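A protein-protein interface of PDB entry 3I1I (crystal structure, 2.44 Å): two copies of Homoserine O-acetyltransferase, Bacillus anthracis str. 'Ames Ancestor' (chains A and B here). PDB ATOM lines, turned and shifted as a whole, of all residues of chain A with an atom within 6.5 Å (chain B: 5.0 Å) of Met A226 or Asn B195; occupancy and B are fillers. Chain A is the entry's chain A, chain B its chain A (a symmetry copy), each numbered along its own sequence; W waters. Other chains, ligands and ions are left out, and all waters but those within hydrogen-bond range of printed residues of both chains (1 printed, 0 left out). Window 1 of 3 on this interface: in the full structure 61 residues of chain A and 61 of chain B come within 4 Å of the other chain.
NE of Arg A225 lies within hydrogen-bond range of OD1 of Asn B195. The guanidinium group (NH1) of Arg A225 is in salt-bridge range of the side-chain carboxylate (OE1) of Glu B198 (2.6 Å). ND2 of Asn A230 sits close to ND2 of Asn B191 (3.1 Å).
The backbone carbonyl oxygen (O) of Val A190 sits at hydrogen-bond distance from the backbone NH (N) of Asn A195 (3.0 Å). ND2 of Asn A195 lies within hydrogen-bond range of OD1 of Asn A191 (3.3 Å). The backbone carbonyl oxygen (O) of Val B190 is in hydrogen-bond range of the backbone NH (N) of Asn B195 (3.0 Å). OD1 of Asn B191 sits at hydrogen-bond distance from ND2 of Asn B195. OE2 of Glu B198 lies within hydrogen-bond range of NE2 of Gln B194, at 2.9 Å. SD of Met B226 is in hydrogen-bond range of N of Ala B196, 3.8 Å away.
Among the printed residues, pairs that only touch across the chains: Met A226 with Met B226 (3.0 Å), Asn A195 with Leu B222 (3.2 Å), Leu A222 with Asn B195 (3.2 Å), Glu A261 with Gln B194 (3.2 Å), Met A229 with Asn B191 (3.3 Å), Arg A225 with Gln B194 (3.5 Å), Arg A225 with Val B190 (3.6 Å), Asn A195 with Met B226 (3.7 Å), Met A226 with Asn B195 (3.7 Å), Met A226 with Asn B191 (3.8 Å), Asn A191 with Met B226 (3.8 Å) and Met A229 with Val B190 (3.8 Å).
Met A226 touches just these residues of chain B: Asn B191, Asn B195 and Met B226. Asn B195 touches just these residues of chain A: Leu A222, Arg A225 and Met A226. Of the printed residues of chain A, Glu B198 touches Arg A225. Printed residues of chain B within 4 Å of Leu A222: Asn B195 (3.2 Å). Of the printed residues of chain A, Val B190 touches Arg A225 (3.6 Å) and Met A229 (3.8 Å). Printed residues of chain A within 4 Å of Asn B191: Met A226 (3.8 Å), Met A229 (3.3 Å) and Asn A230 (3.1 Å). Printed residues of chain A within 4 Å of Gln B194: Arg A225 and Glu A261. The nearest residue of chain A that does not touch Asn B195 is Met A229 (5.1 Å).
Of the 22 printed residues of chain A, 8 touch a printed residue of chain B. Hydrophobic or aromatic side chains of chain A within 4 Å of the printed part of chain B: Leu A222, Met A226 and Met A229. Among the printed residues, Asp or Glu carboxylates within 4 Å of a Lys or Arg side-chain nitrogen of the other chain: Arg A225 with Glu B198 (2.6 Å).
Asn A191 touches Met B226, and with the chains exchanged Met A226 touches Asn B191. Asn A195 touches Leu B222, and with the chains exchanged Leu A222 touches Asn B195. Asn A195 touches Met B226, and with the chains exchanged Met A226 touches Asn B195. Met A226 touches its own counterpart, Met B226. Positions printed for both chains: 190, 191, 192, 194, 195, 196, 197, 199, 222 and 226. Of the 15 pairs that touch across the chains among the printed residues, 7 have their exchanged pair printed and touching as well.
Water W1 lies within hydrogen-bond range of OE1 of Gln B194 (2.7 Å) and O of Glu A261 (3.1 Å).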
ATOM      1  N   VAL A 190      13.064   8.313  26.071  1.00  0.00           N
ATOM      2  CA  VAL A 190      11.812   8.976  25.710  1.00  0.00           C
ATOM      3  C   VAL A 190      11.976   9.820  24.429  1.00  0.00           C
ATOM      4  O   VAL A 190      11.186   9.724  23.473  1.00  0.00           O
ATOM      5  CB  VAL A 190      11.279   9.871  26.869  1.00  0.00           C
ATOM      6  CG1 VAL A 190       9.952  10.495  26.476  1.00  0.00           C
ATOM      7  CG2 VAL A 190      11.169   9.050  28.200  1.00  0.00           C
ATOM      8  N   ASN A 191      13.011  10.646  24.393  1.00  0.00           N
ATOM      9  CA  ASN A 191      13.074  11.647  23.323  1.00  0.00           C
ATOM     10  C   ASN A 191      13.370  11.019  22.003  1.00  0.00           C
ATOM     11  O   ASN A 191      12.869  11.475  21.009  1.00  0.00           O
ATOM     12  CB  ASN A 191      14.077  12.776  23.611  1.00  0.00           C
ATOM     13  CG  ASN A 191      13.533  14.121  23.230  1.00  0.00           C
ATOM     14  OD1 ASN A 191      12.331  14.349  23.272  1.00  0.00           O
ATOM     15  ND2 ASN A 191      14.416  15.031  22.853  1.00  0.00           N
ATOM     16  N   VAL A 192      14.142   9.944  22.000  1.00  0.00           N
ATOM     17  CA  VAL A 192      14.497   9.275  20.765  1.00  0.00           C
ATOM     18  C   VAL A 192      13.876   7.891  20.583  1.00  0.00           C
ATOM     19  O   VAL A 192      13.565   7.542  19.471  1.00  0.00           O
ATOM     20  CB  VAL A 192      16.044   9.219  20.603  1.00  0.00           C
ATOM     21  CG1 VAL A 192      16.434   8.523  19.343  1.00  0.00           C
ATOM     22  CG2 VAL A 192      16.603  10.662  20.652  1.00  0.00           C
ATOM     23  N   GLN A 194      10.908   6.263  22.563  1.00  0.00           N
ATOM     24  CA  GLN A 194       9.446   6.339  22.680  1.00  0.00           C
ATOM     25  C   GLN A 194       8.846   7.236  21.587  1.00  0.00           C
ATOM     26  O   GLN A 194       7.930   6.826  20.867  1.00  0.00           O
ATOM     27  CB  GLN A 194       9.012   6.893  24.042  1.00  0.00           C
ATOM     28  CG  GLN A 194       7.512   6.908  24.203  1.00  0.00           C
ATOM     29  CD  GLN A 194       6.994   7.514  25.489  1.00  0.00           C
ATOM     30  OE1 GLN A 194       7.756   8.025  26.314  1.00  0.00           O
ATOM     31  NE2 GLN A 194       5.663   7.471  25.666  1.00  0.00           N
ATOM     32  N   ASN A 195       9.338   8.466  21.481  1.00  0.00           N
ATOM     33  CA  ASN A 195       8.849   9.377  20.475  1.00  0.00           C
ATOM     34  C   ASN A 195       8.940   8.838  19.042  1.00  0.00           C
ATOM     35  O   ASN A 195       8.036   9.096  18.213  1.00  0.00           O
ATOM     36  CB  ASN A 195       9.545  10.733  20.588  1.00  0.00           C
ATOM     37  CG  ASN A 195       9.069  11.547  21.802  1.00  0.00           C
ATOM     38  OD1 ASN A 195       8.058  11.206  22.445  1.00  0.00           O
ATOM     39  ND2 ASN A 195       9.805  12.618  22.130  1.00  0.00           N
ATOM     40  N   ALA A 196       9.997   8.084  18.748  1.00  0.00           N
ATOM     41  CA  ALA A 196      10.145   7.508  17.396  1.00  0.00           C
ATOM     42  C   ALA A 196       9.088   6.426  17.169  1.00  0.00           C
ATOM     43  O   ALA A 196       8.392   6.419  16.154  1.00  0.00           O
ATOM     44  CB  ALA A 196      11.573   6.939  17.180  1.00  0.00           C
ATOM     45  N   ILE A 197       8.962   5.518  18.127  1.00  0.00           N
ATOM     46  CA  ILE A 197       7.925   4.501  18.051  1.00  0.00           C
ATOM     47  C   ILE A 197       6.546   5.146  17.869  1.00  0.00           C
ATOM     48  O   ILE A 197       5.793   4.776  16.976  1.00  0.00           O
ATOM     49  CB  ILE A 197       7.916   3.617  19.297  1.00  0.00           C
ATOM     50  CG1 ILE A 197       9.230   2.796  19.348  1.00  0.00           C
ATOM     51  CG2 ILE A 197       6.721   2.742  19.268  1.00  0.00           C
ATOM     52  CD1 ILE A 197       9.566   2.145  20.734  1.00  0.00           C
ATOM     53  N   ALA A 199       5.789   8.163  16.731  1.00  0.00           N
ATOM     54  CA  ALA A 199       5.696   8.845  15.436  1.00  0.00           C
ATOM     55  C   ALA A 199       5.313   7.847  14.302  1.00  0.00           C
ATOM     56  O   ALA A 199       4.435   8.121  13.487  1.00  0.00           O
ATOM     57  CB  ALA A 199       7.008   9.594  15.117  1.00  0.00           C
ATOM     58  N   GLN A 221      10.409   8.984   8.659  1.00  0.00           N
ATOM     59  CA  GLN A 221      11.304  10.111   8.520  1.00  0.00           C
ATOM     60  C   GLN A 221      11.373  10.930   9.811  1.00  0.00           C
ATOM     61  O   GLN A 221      12.421  11.409  10.203  1.00  0.00           O
ATOM     62  CB  GLN A 221      10.906  11.033   7.351  1.00  0.00           C
ATOM     63  CG  GLN A 221      11.746  12.360   7.315  1.00  0.00           C
ATOM     64  CD  GLN A 221      11.733  13.064   5.976  1.00  0.00           C
ATOM     65  OE1 GLN A 221      10.759  12.980   5.230  1.00  0.00           O
ATOM     66  NE2 GLN A 221      12.821  13.790   5.666  1.00  0.00           N
ATOM     67  N   LEU A 222      10.237  11.108  10.447  1.00  0.00           N
ATOM     68  CA  LEU A 222      10.182  11.812  11.728  1.00  0.00           C
ATOM     69  C   LEU A 222      10.991  11.050  12.791  1.00  0.00           C
ATOM     70  O   LEU A 222      11.825  11.628  13.487  1.00  0.00           O
ATOM     71  CB  LEU A 222       8.711  12.000  12.115  1.00  0.00           C
ATOM     72  CG  LEU A 222       8.336  12.904  13.266  1.00  0.00           C
ATOM     73  CD1 LEU A 222       9.172  14.192  13.314  1.00  0.00           C
ATOM     74  CD2 LEU A 222       6.825  13.206  13.126  1.00  0.00           C
ATOM     75  N   ALA A 223      10.791   9.738  12.868  1.00  0.00           N
ATOM     76  CA  ALA A 223      11.594   8.889  13.758  1.00  0.00           C
ATOM     77  C   ALA A 223      13.085   9.061  13.483  1.00  0.00           C
ATOM     78  O   ALA A 223      13.868   9.210  14.393  1.00  0.00           O
ATOM     79  CB  ALA A 223      11.163   7.385  13.661  1.00  0.00           C
ATOM     80  N   ASN A 224      13.461   9.076  12.215  1.00  0.00           N
ATOM     81  CA  ASN A 224      14.860   9.173  11.810  1.00  0.00           C
ATOM     82  C   ASN A 224      15.431  10.560  12.090  1.00  0.00           C
ATOM     83  O   ASN A 224      16.575  10.698  12.511  1.00  0.00           O
ATOM     84  CB  ASN A 224      14.975   8.879  10.321  1.00  0.00           C
ATOM     85  CG  ASN A 224      16.431   8.793   9.850  1.00  0.00           C
ATOM     86  OD1 ASN A 224      17.192   7.957  10.313  1.00  0.00           O
ATOM     87  ND2 ASN A 224      16.802   9.648   8.922  1.00  0.00           N
ATOM     88  N   ARG A 225      14.634  11.591  11.858  1.00  0.00           N
ATOM     89  CA  ARG A 225      15.099  12.939  12.115  1.00  0.00           C
ATOM     90  C   ARG A 225      15.381  13.177  13.616  1.00  0.00           C
ATOM     91  O   ARG A 225      16.377  13.790  13.959  1.00  0.00           O
ATOM     92  CB  ARG A 225      14.138  13.982  11.538  1.00  0.00           C
ATOM     93  CG  ARG A 225      14.701  15.365  11.564  1.00  0.00           C
ATOM     94  CD  ARG A 225      14.069  16.298  10.562  1.00  0.00           C
ATOM     95  NE  ARG A 225      12.684  16.431  10.876  1.00  0.00           N
ATOM     96  CZ  ARG A 225      11.676  16.217  10.040  1.00  0.00           C
ATOM     97  NH1 ARG A 225      10.448  16.325  10.502  1.00  0.00           N
ATOM     98  NH2 ARG A 225      11.860  15.903   8.769  1.00  0.00           N
ATOM     99  N   MET A 226      14.553  12.642  14.497  1.00  0.00           N
ATOM    100  CA  MET A 226      14.800  12.739  15.956  1.00  0.00           C
ATOM    101  C   MET A 226      16.120  12.125  16.349  1.00  0.00           C
ATOM    102  O   MET A 226      16.826  12.680  17.151  1.00  0.00           O
ATOM    103  CB  MET A 226      13.714  12.031  16.767  1.00  0.00           C
ATOM    104  CG  MET A 226      12.338  12.678  16.667  1.00  0.00           C
ATOM    105  SD  MET A 226      11.025  11.391  17.267  1.00  0.00           S
ATOM    106  CE  MET A 226       9.435  12.368  16.823  1.00  0.00           C
ATOM    107  N   MET A 227      16.470  10.975  15.800  1.00  0.00           N
ATOM    108  CA  MET A 227      17.771  10.388  16.124  1.00  0.00           C
ATOM    109  C   MET A 227      18.911  11.256  15.545  1.00  0.00           C
ATOM    110  O   MET A 227      19.884  11.574  16.245  1.00  0.00           O
ATOM    111  CB  MET A 227      17.862   8.956  15.599  1.00  0.00           C
ATOM    112  CG  MET A 227      18.884   8.112  16.295  1.00  0.00           C
ATOM    113  SD  MET A 227      18.757   6.222  15.751  1.00  0.00           S
ATOM    114  CE  MET A 227      19.457   6.418  13.956  1.00  0.00           C
ATOM    115  N   PHE A 228      18.779  11.639  14.279  1.00  0.00           N
ATOM    116  CA  PHE A 228      19.802  12.434  13.599  1.00  0.00           C
ATOM    117  C   PHE A 228      20.096  13.747  14.336  1.00  0.00           C
ATOM    118  O   PHE A 228      21.235  14.147  14.482  1.00  0.00           O
ATOM    119  CB  PHE A 228      19.329  12.738  12.155  1.00  0.00           C
ATOM    120  CG  PHE A 228      20.292  13.569  11.387  1.00  0.00           C
ATOM    121  CD1 PHE A 228      21.404  12.973  10.794  1.00  0.00           C
ATOM    122  CD2 PHE A 228      20.138  14.932  11.307  1.00  0.00           C
ATOM    123  CE1 PHE A 228      22.359  13.744  10.108  1.00  0.00           C
ATOM    124  CE2 PHE A 228      21.088  15.742  10.601  1.00  0.00           C
ATOM    125  CZ  PHE A 228      22.194  15.137   9.997  1.00  0.00           C
ATOM    126  N   MET A 229      19.046  14.421  14.784  1.00  0.00           N
ATOM    127  CA  MET A 229      19.233  15.670  15.506  1.00  0.00           C
ATOM    128  C   MET A 229      19.839  15.522  16.912  1.00  0.00           C
ATOM    129  O   MET A 229      20.123  16.524  17.521  1.00  0.00           O
ATOM    130  CB  MET A 229      17.939  16.479  15.625  1.00  0.00           C
ATOM    131  CG  MET A 229      17.328  16.896  14.308  1.00  0.00           C
ATOM    132  SD  MET A 229      18.556  17.853  13.166  1.00  0.00           S
ATOM    133  CE  MET A 229      19.025  19.366  14.377  1.00  0.00           C
ATOM    134  N   ASN A 230      20.083  14.314  17.406  1.00  0.00           N
ATOM    135  CA  ASN A 230      20.882  14.164  18.633  1.00  0.00           C
ATOM    136  C   ASN A 230      22.218  13.461  18.434  1.00  0.00           C
ATOM    137  O   ASN A 230      22.974  13.228  19.409  1.00  0.00           O
ATOM    138  CB  ASN A 230      20.048  13.458  19.708  1.00  0.00           C
ATOM    139  CG  ASN A 230      18.953  14.356  20.258  1.00  0.00           C
ATOM    140  OD1 ASN A 230      19.246  15.350  20.994  1.00  0.00           O
ATOM    141  ND2 ASN A 230      17.683  14.087  19.825  1.00  0.00           N
ATOM    142  N   ALA A 231      22.517  13.159  17.177  1.00  0.00           N
ATOM    143  CA  ALA A 231      23.701  12.362  16.845  1.00  0.00           C
ATOM    144  C   ALA A 231      24.991  13.162  16.900  1.00  0.00           C
ATOM    145  O   ALA A 231      26.041  12.567  17.004  1.00  0.00           O
ATOM    146  CB  ALA A 231      23.539  11.661  15.485  1.00  0.00           C
ATOM    147  N   GLU A 261      15.784  23.302   7.113  1.00  0.00           N
ATOM    148  CA  GLU A 261      14.808  22.226   7.150  1.00  0.00           C
ATOM    149  C   GLU A 261      14.868  21.373   5.879  1.00  0.00           C
ATOM    150  O   GLU A 261      14.760  20.135   5.952  1.00  0.00           O
ATOM    151  CB  GLU A 261      13.399  22.756   7.358  1.00  0.00           C
ATOM    152  CG  GLU A 261      13.078  23.197   8.783  1.00  0.00           C
ATOM    153  CD  GLU A 261      11.728  23.898   8.886  1.00  0.00           C
ATOM    154  OE1 GLU A 261      11.574  25.026   8.352  1.00  0.00           O
ATOM    155  OE2 GLU A 261      10.821  23.305   9.512  1.00  0.00           O
ATOM    156  N   THR A 268      17.555  13.023   5.790  1.00  0.00           N
ATOM    157  CA  THR A 268      16.879  12.070   6.608  1.00  0.00           C
ATOM    158  C   THR A 268      15.936  11.221   5.782  1.00  0.00           C
ATOM    159  O   THR A 268      15.653  10.078   6.156  1.00  0.00           O
ATOM    160  CB  THR A 268      16.137  12.731   7.792  1.00  0.00           C
ATOM    161  OG1 THR A 268      15.222  13.730   7.318  1.00  0.00           O
ATOM    162  CG2 THR A 268      17.116  13.346   8.718  1.00  0.00           C
ATOM    163  N   LEU A 320      23.282  11.731  23.198  1.00  0.00           N
ATOM    164  CA  LEU A 320      22.458  10.503  23.284  1.00  0.00           C
ATOM    165  C   LEU A 320      22.910   9.677  24.453  1.00  0.00           C
ATOM    166  O   LEU A 320      22.096   9.061  25.120  1.00  0.00           O
ATOM    167  CB  LEU A 320      22.548   9.645  22.021  1.00  0.00           C
ATOM    168  CG  LEU A 320      21.792  10.186  20.819  1.00  0.00           C
ATOM    169  CD1 LEU A 320      22.342   9.490  19.563  1.00  0.00           C
ATOM    170  CD2 LEU A 320      20.268   9.980  20.980  1.00  0.00           C
ATOM    171  N   VAL B 190      14.702  22.401  14.636  1.00  0.00           N
ATOM    172  CA  VAL B 190      14.255  21.149  14.028  1.00  0.00           C
ATOM    173  C   VAL B 190      13.712  20.173  15.093  1.00  0.00           C
ATOM    174  O   VAL B 190      12.609  19.613  14.969  1.00  0.00           O
ATOM    175  CB  VAL B 190      15.395  20.464  13.215  1.00  0.00           C
ATOM    176  CG1 VAL B 190      14.875  19.200  12.554  1.00  0.00           C
ATOM    177  CG2 VAL B 190      16.009  21.460  12.172  1.00  0.00           C
ATOM    178  N   ASN B 191      14.477  19.972  16.155  1.00  0.00           N
ATOM    179  CA  ASN B 191      14.137  18.874  17.066  1.00  0.00           C
ATOM    180  C   ASN B 191      12.907  19.178  17.854  1.00  0.00           C
ATOM    181  O   ASN B 191      12.149  18.287  18.130  1.00  0.00           O
ATOM    182  CB  ASN B 191      15.291  18.493  18.009  1.00  0.00           C
ATOM    183  CG  ASN B 191      15.426  17.007  18.157  1.00  0.00           C
ATOM    184  OD1 ASN B 191      15.107  16.251  17.248  1.00  0.00           O
ATOM    185  ND2 ASN B 191      15.904  16.569  19.310  1.00  0.00           N
ATOM    186  N   VAL B 192      12.685  20.445  18.171  1.00  0.00           N
ATOM    187  CA  VAL B 192      11.526  20.835  18.947  1.00  0.00           C
ATOM    188  C   VAL B 192      10.480  21.641  18.179  1.00  0.00           C
ATOM    189  O   VAL B 192       9.316  21.478  18.449  1.00  0.00           O
ATOM    190  CB  VAL B 192      11.964  21.579  20.242  1.00  0.00           C
ATOM    191  CG1 VAL B 192      10.786  22.002  21.052  1.00  0.00           C
ATOM    192  CG2 VAL B 192      12.910  20.658  21.050  1.00  0.00           C
ATOM    193  N   ALA B 193      10.826  22.506  17.237  1.00  0.00           N
ATOM    194  CA  ALA B 193       9.752  23.216  16.484  1.00  0.00           C
ATOM    195  C   ALA B 193       9.243  22.462  15.239  1.00  0.00           C
ATOM    196  O   ALA B 193       8.051  22.187  15.126  1.00  0.00           O
ATOM    197  CB  ALA B 193      10.164  24.638  16.146  1.00  0.00           C
ATOM    198  N   GLN B 194      10.124  22.116  14.303  1.00  0.00           N
ATOM    199  CA  GLN B 194       9.692  21.383  13.104  1.00  0.00           C
ATOM    200  C   GLN B 194       9.029  20.049  13.478  1.00  0.00           C
ATOM    201  O   GLN B 194       7.913  19.754  13.038  1.00  0.00           O
ATOM    202  CB  GLN B 194      10.866  21.086  12.165  1.00  0.00           C
ATOM    203  CG  GLN B 194      10.425  20.398  10.897  1.00  0.00           C
ATOM    204  CD  GLN B 194      11.532  19.996   9.947  1.00  0.00           C
ATOM    205  OE1 GLN B 194      12.720  20.162  10.235  1.00  0.00           O
ATOM    206  NE2 GLN B 194      11.140  19.443   8.787  1.00  0.00           N
ATOM    207  N   ASN B 195       9.725  19.230  14.261  1.00  0.00           N
ATOM    208  CA  ASN B 195       9.180  17.962  14.677  1.00  0.00           C
ATOM    209  C   ASN B 195       7.825  18.062  15.390  1.00  0.00           C
ATOM    210  O   ASN B 195       6.948  17.186  15.203  1.00  0.00           O
ATOM    211  CB  ASN B 195      10.187  17.195  15.535  1.00  0.00           C
ATOM    212  CG  ASN B 195      11.353  16.620  14.715  1.00  0.00           C
ATOM    213  OD1 ASN B 195      11.309  16.596  13.471  1.00  0.00           O
ATOM    214  ND2 ASN B 195      12.408  16.170  15.409  1.00  0.00           N
ATOM    215  N   ALA B 196       7.637  19.117  16.179  1.00  0.00           N
ATOM    216  CA  ALA B 196       6.351  19.299  16.881  1.00  0.00           C
ATOM    217  C   ALA B 196       5.247  19.631  15.876  1.00  0.00           C
ATOM    218  O   ALA B 196       4.176  19.026  15.883  1.00  0.00           O
ATOM    219  CB  ALA B 196       6.455  20.399  17.972  1.00  0.00           C
ATOM    220  N   ILE B 197       5.520  20.590  15.001  1.00  0.00           N
ATOM    221  CA  ILE B 197       4.574  20.920  13.947  1.00  0.00           C
ATOM    222  C   ILE B 197       4.211  19.670  13.135  1.00  0.00           C
ATOM    223  O   ILE B 197       3.039  19.374  12.931  1.00  0.00           O
ATOM    224  CB  ILE B 197       5.130  21.994  13.012  1.00  0.00           C
ATOM    225  CG1 ILE B 197       5.280  23.322  13.797  1.00  0.00           C
ATOM    226  CG2 ILE B 197       4.229  22.142  11.846  1.00  0.00           C
ATOM    227  CD1 ILE B 197       6.190  24.405  13.122  1.00  0.00           C
ATOM    228  N   GLU B 198       5.210  18.932  12.687  1.00  0.00           N
ATOM    229  CA  GLU B 198       4.930  17.731  11.924  1.00  0.00           C
ATOM    230  C   GLU B 198       4.192  16.629  12.701  1.00  0.00           C
ATOM    231  O   GLU B 198       3.352  15.958  12.132  1.00  0.00           O
ATOM    232  CB  GLU B 198       6.206  17.214  11.268  1.00  0.00           C
ATOM    233  CG  GLU B 198       6.482  18.095  10.037  1.00  0.00           C
ATOM    234  CD  GLU B 198       7.746  17.757   9.305  1.00  0.00           C
ATOM    235  OE1 GLU B 198       8.136  16.556   9.336  1.00  0.00           O
ATOM    236  OE2 GLU B 198       8.313  18.695   8.661  1.00  0.00           O
ATOM    237  N   ALA B 199       4.469  16.481  13.988  1.00  0.00           N
ATOM    238  CA  ALA B 199       3.739  15.513  14.814  1.00  0.00           C
ATOM    239  C   ALA B 199       2.218  15.851  14.862  1.00  0.00           C
ATOM    240  O   ALA B 199       1.370  14.978  14.693  1.00  0.00           O
ATOM    241  CB  ALA B 199       4.350  15.431  16.230  1.00  0.00           C
ATOM    242  N   LEU B 222       2.629  14.440  21.760  1.00  0.00           N
ATOM    243  CA  LEU B 222       3.956  14.178  21.205  1.00  0.00           C
ATOM    244  C   LEU B 222       4.740  15.491  21.050  1.00  0.00           C
ATOM    245  O   LEU B 222       5.886  15.601  21.484  1.00  0.00           O
ATOM    246  CB  LEU B 222       3.787  13.421  19.883  1.00  0.00           C
ATOM    247  CG  LEU B 222       4.986  12.802  19.201  1.00  0.00           C
ATOM    248  CD1 LEU B 222       5.962  12.142  20.187  1.00  0.00           C
ATOM    249  CD2 LEU B 222       4.441  11.787  18.168  1.00  0.00           C
ATOM    250  N   MET B 226       8.216  16.340  23.359  1.00  0.00           N
ATOM    251  CA  MET B 226       9.509  16.776  22.778  1.00  0.00           C
ATOM    252  C   MET B 226      10.030  18.029  23.436  1.00  0.00           C
ATOM    253  O   MET B 226      11.201  18.125  23.704  1.00  0.00           O
ATOM    254  CB  MET B 226       9.393  17.067  21.282  1.00  0.00           C
ATOM    255  CG  MET B 226       9.097  15.840  20.428  1.00  0.00           C
ATOM    256  SD  MET B 226       8.449  16.448  18.709  1.00  0.00           S
ATOM    257  CE  MET B 226       7.958  14.749  17.966  1.00  0.00           C
HETATM  258  O   HOH W   1      14.556  18.825   8.708  1.00  0.00           O
